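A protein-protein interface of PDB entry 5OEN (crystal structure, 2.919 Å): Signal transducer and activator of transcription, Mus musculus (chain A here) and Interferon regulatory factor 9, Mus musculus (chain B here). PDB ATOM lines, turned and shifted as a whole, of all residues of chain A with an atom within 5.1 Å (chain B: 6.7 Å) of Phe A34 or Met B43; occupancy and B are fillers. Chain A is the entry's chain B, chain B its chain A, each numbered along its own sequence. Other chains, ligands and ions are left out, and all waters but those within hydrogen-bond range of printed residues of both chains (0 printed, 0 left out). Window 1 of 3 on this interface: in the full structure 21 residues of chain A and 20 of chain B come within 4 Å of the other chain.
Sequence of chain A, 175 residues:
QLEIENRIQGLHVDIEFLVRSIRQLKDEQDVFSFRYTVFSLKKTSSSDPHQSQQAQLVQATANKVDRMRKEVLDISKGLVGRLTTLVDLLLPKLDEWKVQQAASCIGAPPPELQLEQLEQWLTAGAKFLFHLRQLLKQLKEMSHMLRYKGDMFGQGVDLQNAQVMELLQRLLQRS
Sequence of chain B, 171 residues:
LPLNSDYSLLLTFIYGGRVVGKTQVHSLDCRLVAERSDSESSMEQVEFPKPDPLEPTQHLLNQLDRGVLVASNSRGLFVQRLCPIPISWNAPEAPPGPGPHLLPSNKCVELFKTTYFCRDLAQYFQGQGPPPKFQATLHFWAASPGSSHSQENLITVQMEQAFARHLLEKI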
ATOM      1  N   GLU A  28     -31.265  14.277 -27.518  1.00  0.00           N
ATOM      2  CA  GLU A  28     -30.549  13.559 -28.567  1.00  0.00           C
ATOM      3  C   GLU A  28     -29.319  14.314 -29.053  1.00  0.00           C
ATOM      4  O   GLU A  28     -28.323  13.684 -29.423  1.00  0.00           O
ATOM      5  CB  GLU A  28     -31.486  13.275 -29.739  1.00  0.00           C
ATOM      6  CG  GLU A  28     -32.154  11.912 -29.665  1.00  0.00           C
ATOM      7  CD  GLU A  28     -31.322  10.817 -30.304  1.00  0.00           C
ATOM      8  OE1 GLU A  28     -30.732  11.067 -31.375  1.00  0.00           O
ATOM      9  OE2 GLU A  28     -31.253   9.708 -29.733  1.00  0.00           O
ATOM     10  N   ASP A  30     -27.318  15.917 -27.222  1.00  0.00           N
ATOM     11  CA  ASP A  30     -26.280  15.496 -26.287  1.00  0.00           C
ATOM     12  C   ASP A  30     -25.729  14.126 -26.665  1.00  0.00           C
ATOM     13  O   ASP A  30     -24.512  13.905 -26.625  1.00  0.00           O
ATOM     14  CB  ASP A  30     -26.831  15.467 -24.861  1.00  0.00           C
ATOM     15  CG  ASP A  30     -27.268  16.836 -24.368  1.00  0.00           C
ATOM     16  OD1 ASP A  30     -26.679  17.849 -24.801  1.00  0.00           O
ATOM     17  OD2 ASP A  30     -28.202  16.897 -23.539  1.00  0.00           O
ATOM     18  N   VAL A  31     -26.613  13.193 -27.030  1.00  0.00           N
ATOM     19  CA  VAL A  31     -26.185  11.857 -27.444  1.00  0.00           C
ATOM     20  C   VAL A  31     -25.166  11.955 -28.573  1.00  0.00           C
ATOM     21  O   VAL A  31     -24.077  11.372 -28.507  1.00  0.00           O
ATOM     22  CB  VAL A  31     -27.405  11.012 -27.855  1.00  0.00           C
ATOM     23  CG1 VAL A  31     -26.977   9.681 -28.462  1.00  0.00           C
ATOM     24  CG2 VAL A  31     -28.317  10.783 -26.655  1.00  0.00           C
ATOM     25  N   PHE A  32     -25.503  12.703 -29.624  1.00  0.00           N
ATOM     26  CA  PHE A  32     -24.628  12.785 -30.789  1.00  0.00           C
ATOM     27  C   PHE A  32     -23.244  13.288 -30.401  1.00  0.00           C
ATOM     28  O   PHE A  32     -22.231  12.649 -30.706  1.00  0.00           O
ATOM     29  CB  PHE A  32     -25.252  13.691 -31.852  1.00  0.00           C
ATOM     30  CG  PHE A  32     -24.300  14.079 -32.948  1.00  0.00           C
ATOM     31  CD1 PHE A  32     -24.076  13.234 -34.021  1.00  0.00           C
ATOM     32  CD2 PHE A  32     -23.624  15.285 -32.900  1.00  0.00           C
ATOM     33  CE1 PHE A  32     -23.196  13.587 -35.028  1.00  0.00           C
ATOM     34  CE2 PHE A  32     -22.745  15.643 -33.903  1.00  0.00           C
ATOM     35  CZ  PHE A  32     -22.530  14.792 -34.967  1.00  0.00           C
ATOM     36  N   SER A  33     -23.181  14.435 -29.721  1.00  0.00           N
ATOM     37  CA  SER A  33     -21.886  15.016 -29.378  1.00  0.00           C
ATOM     38  C   SER A  33     -21.084  14.086 -28.478  1.00  0.00           C
ATOM     39  O   SER A  33     -19.853  14.024 -28.576  1.00  0.00           O
ATOM     40  CB  SER A  33     -22.085  16.375 -28.707  1.00  0.00           C
ATOM     41  OG  SER A  33     -22.918  16.260 -27.567  1.00  0.00           O
ATOM     42  N   PHE A  34     -21.763  13.358 -27.589  1.00  0.00           N
ATOM     43  CA  PHE A  34     -21.082  12.369 -26.760  1.00  0.00           C
ATOM     44  C   PHE A  34     -20.475  11.271 -27.624  1.00  0.00           C
ATOM     45  O   PHE A  34     -19.268  11.008 -27.567  1.00  0.00           O
ATOM     46  CB  PHE A  34     -22.058  11.781 -25.739  1.00  0.00           C
ATOM     47  CG  PHE A  34     -21.497  10.624 -24.958  1.00  0.00           C
ATOM     48  CD1 PHE A  34     -20.535  10.830 -23.981  1.00  0.00           C
ATOM     49  CD2 PHE A  34     -21.935   9.330 -25.193  1.00  0.00           C
ATOM     50  CE1 PHE A  34     -20.018   9.769 -23.261  1.00  0.00           C
ATOM     51  CE2 PHE A  34     -21.422   8.266 -24.474  1.00  0.00           C
ATOM     52  CZ  PHE A  34     -20.463   8.486 -23.507  1.00  0.00           C
ATOM     53  N   ARG A  35     -21.305  10.618 -28.440  1.00  0.00           N
ATOM     54  CA  ARG A  35     -20.798   9.604 -29.357  1.00  0.00           C
ATOM     55  C   ARG A  35     -19.753  10.184 -30.299  1.00  0.00           C
ATOM     56  O   ARG A  35     -18.717   9.558 -30.550  1.00  0.00           O
ATOM     57  CB  ARG A  35     -21.951   9.000 -30.155  1.00  0.00           C
ATOM     58  CG  ARG A  35     -22.973   8.282 -29.307  1.00  0.00           C
ATOM     59  CD  ARG A  35     -24.064   7.681 -30.170  1.00  0.00           C
ATOM     60  NE  ARG A  35     -25.041   6.927 -29.389  1.00  0.00           N
ATOM     61  CZ  ARG A  35     -26.132   6.369 -29.902  1.00  0.00           C
ATOM     62  NH1 ARG A  35     -26.391   6.479 -31.199  1.00  0.00           N
ATOM     63  NH2 ARG A  35     -26.968   5.703 -29.119  1.00  0.00           N
ATOM     64  N   TYR A  36     -20.017  11.373 -30.845  1.00  0.00           N
ATOM     65  CA  TYR A  36     -19.051  12.012 -31.732  1.00  0.00           C
ATOM     66  C   TYR A  36     -17.705  12.174 -31.037  1.00  0.00           C
ATOM     67  O   TYR A  36     -16.658  11.822 -31.591  1.00  0.00           O
ATOM     68  CB  TYR A  36     -19.593  13.368 -32.194  1.00  0.00           C
ATOM     69  CG  TYR A  36     -18.898  13.962 -33.403  1.00  0.00           C
ATOM     70  CD1 TYR A  36     -18.770  15.340 -33.548  1.00  0.00           C
ATOM     71  CD2 TYR A  36     -18.395  13.153 -34.411  1.00  0.00           C
ATOM     72  CE1 TYR A  36     -18.146  15.890 -34.655  1.00  0.00           C
ATOM     73  CE2 TYR A  36     -17.771  13.693 -35.519  1.00  0.00           C
ATOM     74  CZ  TYR A  36     -17.649  15.059 -35.638  1.00  0.00           C
ATOM     75  OH  TYR A  36     -17.028  15.590 -36.746  1.00  0.00           O
ATOM     76  N   THR A  37     -17.719  12.701 -29.811  1.00  0.00           N
ATOM     77  CA  THR A  37     -16.479  12.879 -29.063  1.00  0.00           C
ATOM     78  C   THR A  37     -15.802  11.538 -28.803  1.00  0.00           C
ATOM     79  O   THR A  37     -14.592  11.390 -29.017  1.00  0.00           O
ATOM     80  CB  THR A  37     -16.763  13.604 -27.745  1.00  0.00           C
ATOM     81  OG1 THR A  37     -17.381  14.870 -28.015  1.00  0.00           O
ATOM     82  CG2 THR A  37     -15.473  13.833 -26.960  1.00  0.00           C
ATOM     83  N   VAL A  38     -16.567  10.547 -28.338  1.00  0.00           N
ATOM     84  CA  VAL A  38     -16.000   9.226 -28.079  1.00  0.00           C
ATOM     85  C   VAL A  38     -15.380   8.660 -29.350  1.00  0.00           C
ATOM     86  O   VAL A  38     -14.279   8.098 -29.324  1.00  0.00           O
ATOM     87  CB  VAL A  38     -17.076   8.287 -27.501  1.00  0.00           C
ATOM     88  CG1 VAL A  38     -16.583   6.839 -27.463  1.00  0.00           C
ATOM     89  CG2 VAL A  38     -17.472   8.743 -26.104  1.00  0.00           C
ATOM     90  N   PHE A  39     -16.074   8.800 -30.481  1.00  0.00           N
ATOM     91  CA  PHE A  39     -15.517   8.343 -31.748  1.00  0.00           C
ATOM     92  C   PHE A  39     -14.216   9.064 -32.076  1.00  0.00           C
ATOM     93  O   PHE A  39     -13.301   8.461 -32.646  1.00  0.00           O
ATOM     94  CB  PHE A  39     -16.538   8.544 -32.868  1.00  0.00           C
ATOM     95  CG  PHE A  39     -15.998   8.264 -34.241  1.00  0.00           C
ATOM     96  CD1 PHE A  39     -15.674   9.301 -35.095  1.00  0.00           C
ATOM     97  CD2 PHE A  39     -15.816   6.965 -34.676  1.00  0.00           C
ATOM     98  CE1 PHE A  39     -15.179   9.049 -36.357  1.00  0.00           C
ATOM     99  CE2 PHE A  39     -15.320   6.706 -35.935  1.00  0.00           C
ATOM    100  CZ  PHE A  39     -15.003   7.750 -36.776  1.00  0.00           C
ATOM    101  N   SER B  27     -25.055  -3.171 -25.215  1.00  0.00           N
ATOM    102  CA  SER B  27     -25.018  -2.119 -26.220  1.00  0.00           C
ATOM    103  C   SER B  27     -23.782  -1.249 -26.035  1.00  0.00           C
ATOM    104  O   SER B  27     -23.228  -1.145 -24.938  1.00  0.00           O
ATOM    105  CB  SER B  27     -26.278  -1.256 -26.147  1.00  0.00           C
ATOM    106  OG  SER B  27     -26.264  -0.251 -27.146  1.00  0.00           O
ATOM    107  N   LEU B  28     -23.349  -0.623 -27.134  1.00  0.00           N
ATOM    108  CA  LEU B  28     -22.191   0.262 -27.074  1.00  0.00           C
ATOM    109  C   LEU B  28     -22.414   1.414 -26.107  1.00  0.00           C
ATOM    110  O   LEU B  28     -21.457   1.909 -25.501  1.00  0.00           O
ATOM    111  CB  LEU B  28     -21.874   0.812 -28.466  1.00  0.00           C
ATOM    112  CG  LEU B  28     -21.377  -0.175 -29.521  1.00  0.00           C
ATOM    113  CD1 LEU B  28     -21.201   0.543 -30.850  1.00  0.00           C
ATOM    114  CD2 LEU B  28     -20.075  -0.829 -29.091  1.00  0.00           C
ATOM    115  N   ASP B  29     -23.659   1.855 -25.952  1.00  0.00           N
ATOM    116  CA  ASP B  29     -23.979   3.009 -25.131  1.00  0.00           C
ATOM    117  C   ASP B  29     -25.137   2.682 -24.202  1.00  0.00           C
ATOM    118  O   ASP B  29     -25.865   1.704 -24.393  1.00  0.00           O
ATOM    119  CB  ASP B  29     -24.355   4.229 -25.980  1.00  0.00           C
ATOM    120  CG  ASP B  29     -23.200   4.752 -26.811  1.00  0.00           C
ATOM    121  OD1 ASP B  29     -22.032   4.511 -26.442  1.00  0.00           O
ATOM    122  OD2 ASP B  29     -23.467   5.413 -27.836  1.00  0.00           O
ATOM    123  N   CYS B  30     -25.296   3.531 -23.192  1.00  0.00           N
ATOM    124  CA  CYS B  30     -26.445   3.485 -22.303  1.00  0.00           C
ATOM    125  C   CYS B  30     -26.482   4.790 -21.525  1.00  0.00           C
ATOM    126  O   CYS B  30     -25.474   5.493 -21.411  1.00  0.00           O
ATOM    127  CB  CYS B  30     -26.384   2.288 -21.349  1.00  0.00           C
ATOM    128  SG  CYS B  30     -25.305   2.517 -19.921  1.00  0.00           S
ATOM    129  N   ARG B  31     -27.662   5.111 -21.006  1.00  0.00           N
ATOM    130  CA  ARG B  31     -27.845   6.264 -20.136  1.00  0.00           C
ATOM    131  C   ARG B  31     -28.496   5.794 -18.846  1.00  0.00           C
ATOM    132  O   ARG B  31     -29.537   5.130 -18.875  1.00  0.00           O
ATOM    133  CB  ARG B  31     -28.695   7.349 -20.803  1.00  0.00           C
ATOM    134  CG  ARG B  31     -28.860   8.601 -19.950  1.00  0.00           C
ATOM    135  CD  ARG B  31     -29.039   9.851 -20.795  1.00  0.00           C
ATOM    136  NE  ARG B  31     -30.381   9.982 -21.354  1.00  0.00           N
ATOM    137  CZ  ARG B  31     -30.702  10.854 -22.306  1.00  0.00           C
ATOM    138  NH1 ARG B  31     -29.783  11.670 -22.810  1.00  0.00           N
ATOM    139  NH2 ARG B  31     -31.946  10.908 -22.762  1.00  0.00           N
ATOM    140  N   GLU B  40     -37.977   8.989 -28.242  1.00  0.00           N
ATOM    141  CA  GLU B  40     -37.333   8.137 -29.240  1.00  0.00           C
ATOM    142  C   GLU B  40     -35.849   8.484 -29.245  1.00  0.00           C
ATOM    143  O   GLU B  40     -35.394   9.346 -29.996  1.00  0.00           O
ATOM    144  CB  GLU B  40     -37.964   8.327 -30.616  1.00  0.00           C
ATOM    145  CG  GLU B  40     -37.213   7.629 -31.743  1.00  0.00           C
ATOM    146  CD  GLU B  40     -36.961   6.161 -31.453  1.00  0.00           C
ATOM    147  OE1 GLU B  40     -37.814   5.532 -30.794  1.00  0.00           O
ATOM    148  OE2 GLU B  40     -35.909   5.639 -31.879  1.00  0.00           O
ATOM    149  N   SER B  41     -35.091   7.805 -28.392  1.00  0.00           N
ATOM    150  CA  SER B  41     -33.651   7.998 -28.289  1.00  0.00           C
ATOM    151  C   SER B  41     -32.939   6.779 -28.858  1.00  0.00           C
ATOM    152  O   SER B  41     -33.271   5.641 -28.512  1.00  0.00           O
ATOM    153  CB  SER B  41     -33.229   8.229 -26.837  1.00  0.00           C
ATOM    154  OG  SER B  41     -31.837   8.473 -26.745  1.00  0.00           O
ATOM    155  N   SER B  42     -31.961   7.023 -29.730  1.00  0.00           N
ATOM    156  CA  SER B  42     -31.162   5.934 -30.277  1.00  0.00           C
ATOM    157  C   SER B  42     -30.387   5.200 -29.194  1.00  0.00           C
ATOM    158  O   SER B  42     -30.022   4.036 -29.387  1.00  0.00           O
ATOM    159  CB  SER B  42     -30.200   6.478 -31.333  1.00  0.00           C
ATOM    160  OG  SER B  42     -29.398   7.519 -30.801  1.00  0.00           O
ATOM    161  N   MET B  43     -30.132   5.848 -28.062  1.00  0.00           N
ATOM    162  CA  MET B  43     -29.329   5.259 -27.001  1.00  0.00           C
ATOM    163  C   MET B  43     -30.210   4.545 -25.986  1.00  0.00           C
ATOM    164  O   MET B  43     -31.299   5.018 -25.647  1.00  0.00           O
ATOM    165  CB  MET B  43     -28.509   6.336 -26.289  1.00  0.00           C
ATOM    166  CG  MET B  43     -27.376   5.768 -25.454  1.00  0.00           C
ATOM    167  SD  MET B  43     -26.601   6.966 -24.355  1.00  0.00           S
ATOM    168  CE  MET B  43     -25.372   7.697 -25.436  1.00  0.00           C
ATOM    169  N   GLU B  44     -29.723   3.409 -25.493  1.00  0.00           N
ATOM    170  CA  GLU B  44     -30.436   2.665 -24.466  1.00  0.00           C
ATOM    171  C   GLU B  44     -30.452   3.450 -23.159  1.00  0.00           C
ATOM    172  O   GLU B  44     -29.545   4.237 -22.868  1.00  0.00           O
ATOM    173  CB  GLU B  44     -29.784   1.298 -24.246  1.00  0.00           C
ATOM    174  CG  GLU B  44     -30.563   0.370 -23.320  1.00  0.00           C
ATOM    175  CD  GLU B  44     -29.780  -0.870 -22.942  1.00  0.00           C
ATOM    176  OE1 GLU B  44     -28.779  -1.177 -23.623  1.00  0.00           O
ATOM    177  OE2 GLU B  44     -30.167  -1.533 -21.956  1.00  0.00           O
ATOM    178  N   GLN B  45     -31.499   3.231 -22.367  1.00  0.00           N
ATOM    179  CA  GLN B  45     -31.665   3.879 -21.071  1.00  0.00           C
ATOM    180  C   GLN B  45     -31.827   2.806 -20.004  1.00  0.00           C
ATOM    181  O   GLN B  45     -32.734   1.971 -20.090  1.00  0.00           O
ATOM    182  CB  GLN B  45     -32.870   4.824 -21.078  1.00  0.00           C
ATOM    183  CG  GLN B  45     -32.668   6.067 -21.933  1.00  0.00           C
ATOM    184  CD  GLN B  45     -33.807   7.062 -21.805  1.00  0.00           C
ATOM    185  OE1 GLN B  45     -33.583   8.257 -21.615  1.00  0.00           O
ATOM    186  NE2 GLN B  45     -35.036   6.573 -21.915  1.00  0.00           N
ATOM    187  N   VAL B  68     -26.528  10.055 -16.496  1.00  0.00           N
ATOM    188  CA  VAL B  68     -25.129   9.785 -16.807  1.00  0.00           C
ATOM    189  C   VAL B  68     -25.061   8.979 -18.096  1.00  0.00           C
ATOM    190  O   VAL B  68     -25.855   8.055 -18.306  1.00  0.00           O
ATOM    191  CB  VAL B  68     -24.426   9.027 -15.662  1.00  0.00           C
ATOM    192  CG1 VAL B  68     -22.941   8.859 -15.961  1.00  0.00           C
ATOM    193  CG2 VAL B  68     -24.627   9.749 -14.341  1.00  0.00           C
ATOM    194  N   LEU B  69     -24.100   9.325 -18.948  1.00  0.00           N
ATOM    195  CA  LEU B  69     -23.835   8.610 -20.189  1.00  0.00           C
ATOM    196  C   LEU B  69     -22.590   7.751 -20.020  1.00  0.00           C
ATOM    197  O   LEU B  69     -21.547   8.246 -19.583  1.00  0.00           O
ATOM    198  CB  LEU B  69     -23.628   9.586 -21.349  1.00  0.00           C
ATOM    199  CG  LEU B  69     -24.810  10.464 -21.747  1.00  0.00           C
ATOM    200  CD1 LEU B  69     -24.375  11.469 -22.790  1.00  0.00           C
ATOM    201  CD2 LEU B  69     -25.925   9.614 -22.291  1.00  0.00           C
ATOM    202  N   VAL B  70     -22.696   6.473 -20.376  1.00  0.00           N
ATOM    203  CA  VAL B  70     -21.571   5.547 -20.321  1.00  0.00           C
ATOM    204  C   VAL B  70     -21.419   4.890 -21.686  1.00  0.00           C
ATOM    205  O   VAL B  70     -22.405   4.426 -22.269  1.00  0.00           O
ATOM    206  CB  VAL B  70     -21.754   4.479 -19.227  1.00  0.00           C
ATOM    207  CG1 VAL B  70     -20.469   3.677 -19.058  1.00  0.00           C
ATOM    208  CG2 VAL B  70     -22.167   5.126 -17.910  1.00  0.00           C
ATOM    209  N   ALA B  71     -20.185   4.846 -22.189  1.00  0.00           N
ATOM    210  CA  ALA B  71     -19.866   4.211 -23.461  1.00  0.00           C
ATOM    211  C   ALA B  71     -18.886   3.076 -23.210  1.00  0.00           C
ATOM    212  O   ALA B  71     -17.783   3.305 -22.702  1.00  0.00           O
ATOM    213  CB  ALA B  71     -19.273   5.218 -24.447  1.00  0.00           C
ATOM    214  N   PHE B  78     -16.008   5.087 -21.289  1.00  0.00           N
ATOM    215  CA  PHE B  78     -16.100   6.535 -21.330  1.00  0.00           C
ATOM    216  C   PHE B  78     -17.379   6.956 -20.626  1.00  0.00           C
ATOM    217  O   PHE B  78     -18.388   6.246 -20.668  1.00  0.00           O
ATOM    218  CB  PHE B  78     -16.103   7.076 -22.770  1.00  0.00           C
ATOM    219  CG  PHE B  78     -15.105   6.410 -23.678  1.00  0.00           C
ATOM    220  CD1 PHE B  78     -15.343   5.139 -24.177  1.00  0.00           C
ATOM    221  CD2 PHE B  78     -13.942   7.062 -24.049  1.00  0.00           C
ATOM    222  CE1 PHE B  78     -14.433   4.529 -25.015  1.00  0.00           C
ATOM    223  CE2 PHE B  78     -13.029   6.455 -24.891  1.00  0.00           C
ATOM    224  CZ  PHE B  78     -13.276   5.188 -25.374  1.00  0.00           C
ATOM    225  N   VAL B  79     -17.336   8.117 -19.977  1.00  0.00           N
ATOM    226  CA  VAL B  79     -18.474   8.612 -19.215  1.00  0.00           C
ATOM    227  C   VAL B  79     -18.598  10.115 -19.416  1.00  0.00           C
ATOM    228  O   VAL B  79     -17.604  10.819 -19.613  1.00  0.00           O
ATOM    229  CB  VAL B  79     -18.345   8.276 -17.711  1.00  0.00           C
ATOM    230  CG1 VAL B  79     -17.159   9.007 -17.091  1.00  0.00           C
ATOM    231  CG2 VAL B  79     -19.634   8.602 -16.969  1.00  0.00           C
ATOM    232  N   GLN B  80     -19.838  10.604 -19.369  1.00  0.00           N
ATOM    233  CA  GLN B  80     -20.107  12.035 -19.331  1.00  0.00           C
ATOM    234  C   GLN B  80     -21.241  12.300 -18.355  1.00  0.00           C
ATOM    235  O   GLN B  80     -22.295  11.663 -18.437  1.00  0.00           O
ATOM    236  CB  GLN B  80     -20.469  12.585 -20.712  1.00  0.00           C
ATOM    237  CG  GLN B  80     -20.694  14.089 -20.709  1.00  0.00           C
ATOM    238  CD  GLN B  80     -20.898  14.657 -22.095  1.00  0.00           C
ATOM    239  OE1 GLN B  80     -20.763  13.952 -23.095  1.00  0.00           O
ATOM    240  NE2 GLN B  80     -21.227  15.941 -22.162  1.00  0.00           N
ATOM    241  N   CYS B 108     -16.254  14.778 -21.856  1.00  0.00           N
ATOM    242  CA  CYS B 108     -16.218  13.321 -21.885  1.00  0.00           C
ATOM    243  C   CYS B 108     -14.934  12.831 -21.226  1.00  0.00           C
ATOM    244  O   CYS B 108     -13.834  13.213 -21.641  1.00  0.00           O
ATOM    245  CB  CYS B 108     -16.315  12.816 -23.324  1.00  0.00           C
ATOM    246  SG  CYS B 108     -16.398  11.015 -23.475  1.00  0.00           S
ATOM    247  N   VAL B 109     -15.076  11.981 -20.212  1.00  0.00           N
ATOM    248  CA  VAL B 109     -13.959  11.511 -19.399  1.00  0.00           C
ATOM    249  C   VAL B 109     -13.684  10.054 -19.747  1.00  0.00           C
ATOM    250  O   VAL B 109     -14.610   9.234 -19.792  1.00  0.00           O
ATOM    251  CB  VAL B 109     -14.258  11.675 -17.898  1.00  0.00           C
ATOM    252  CG1 VAL B 109     -13.090  11.179 -17.054  1.00  0.00           C
ATOM    253  CG2 VAL B 109     -14.578  13.129 -17.577  1.00  0.00           C
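The backbone NH (N) of Ser B42 sits at hydrogen-bond distance from the side-chain carboxylate (OE2) of Glu A28 (2.8 Å). NH2 of Arg A35 sits close to N of Met B43, 3.3 Å away. The side-chain carboxylate (OD2) of Asp B29 is in salt-bridge range of the guanidinium group (NE) of Arg A35, at 2.7 Å. OG of Ser B42 sits at hydrogen-bond distance from NH1 of Arg A35. The side-chain hydroxyl of Ser B41 lies close to the side-chain carboxylate of Glu A28.
O of Phe B78 is in hydrogen-bond range of N of Ala B71, 2.7 Å away. OG of Ser B27 sits at hydrogen-bond distance from O of Asp B29 (3.4 Å). The side-chain hydroxyl (OG1) of Thr A37 is in hydrogen-bond range of the backbone carbonyl oxygen (O) of Ser A33. The side-chain hydroxyl of Ser B41 lies close to the backbone NH of Met B43 (3.4 Å). O of Leu B69 lies within hydrogen-bond range of N of Gln B80, at 2.9 Å.
Among the printed residues, pairs that only touch across the chains: Phe A34 with Gln B80, Phe A34 with Ala B71, Val A38 with Cys B108, Phe A34 with Leu B69, Phe A34 with Met B43, Phe A34 with Cys B108, Thr A37 with Cys B108, Val A38 with Phe B78 and Val A31 with Met B43.
Of the printed residues of chain B, Glu A28 touches Ser B41 and Ser B42. Phe A34 touches just these residues of chain B: Met B43 (3.8 Å), Leu B69 (3.7 Å), Ala B71 (3.6 Å), Gln B80 (3.3 Å) and Cys B108 (3.8 Å). Of the printed residues of chain A, Ser B42 touches Glu A28 (2.8 Å) and Arg A35 (3.2 Å). Of chain A, only Val A31 (3.96 Å), Phe A34 (3.8 Å) and Arg A35 (3.2 Å) come within 4 Å of Met B43. The nearest residue of chain A that does not touch Met B43 is Glu A28 (4.4 Å).
Hydrophobic or aromatic side chains of chain B that line the printed part of chain A: Met B43, Leu B69, Ala B71 and Phe B78. Printed residues of chain A that touch a printed residue of chain B: Glu A28, Val A31, Phe A34, Arg A35, Thr A37 and Val A38. Hydrophobic or aromatic side chains of chain A that line the printed part of chain B: Val A31, Phe A34 and Val A38. Among the printed residues, 14 pairs touch across the chains.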
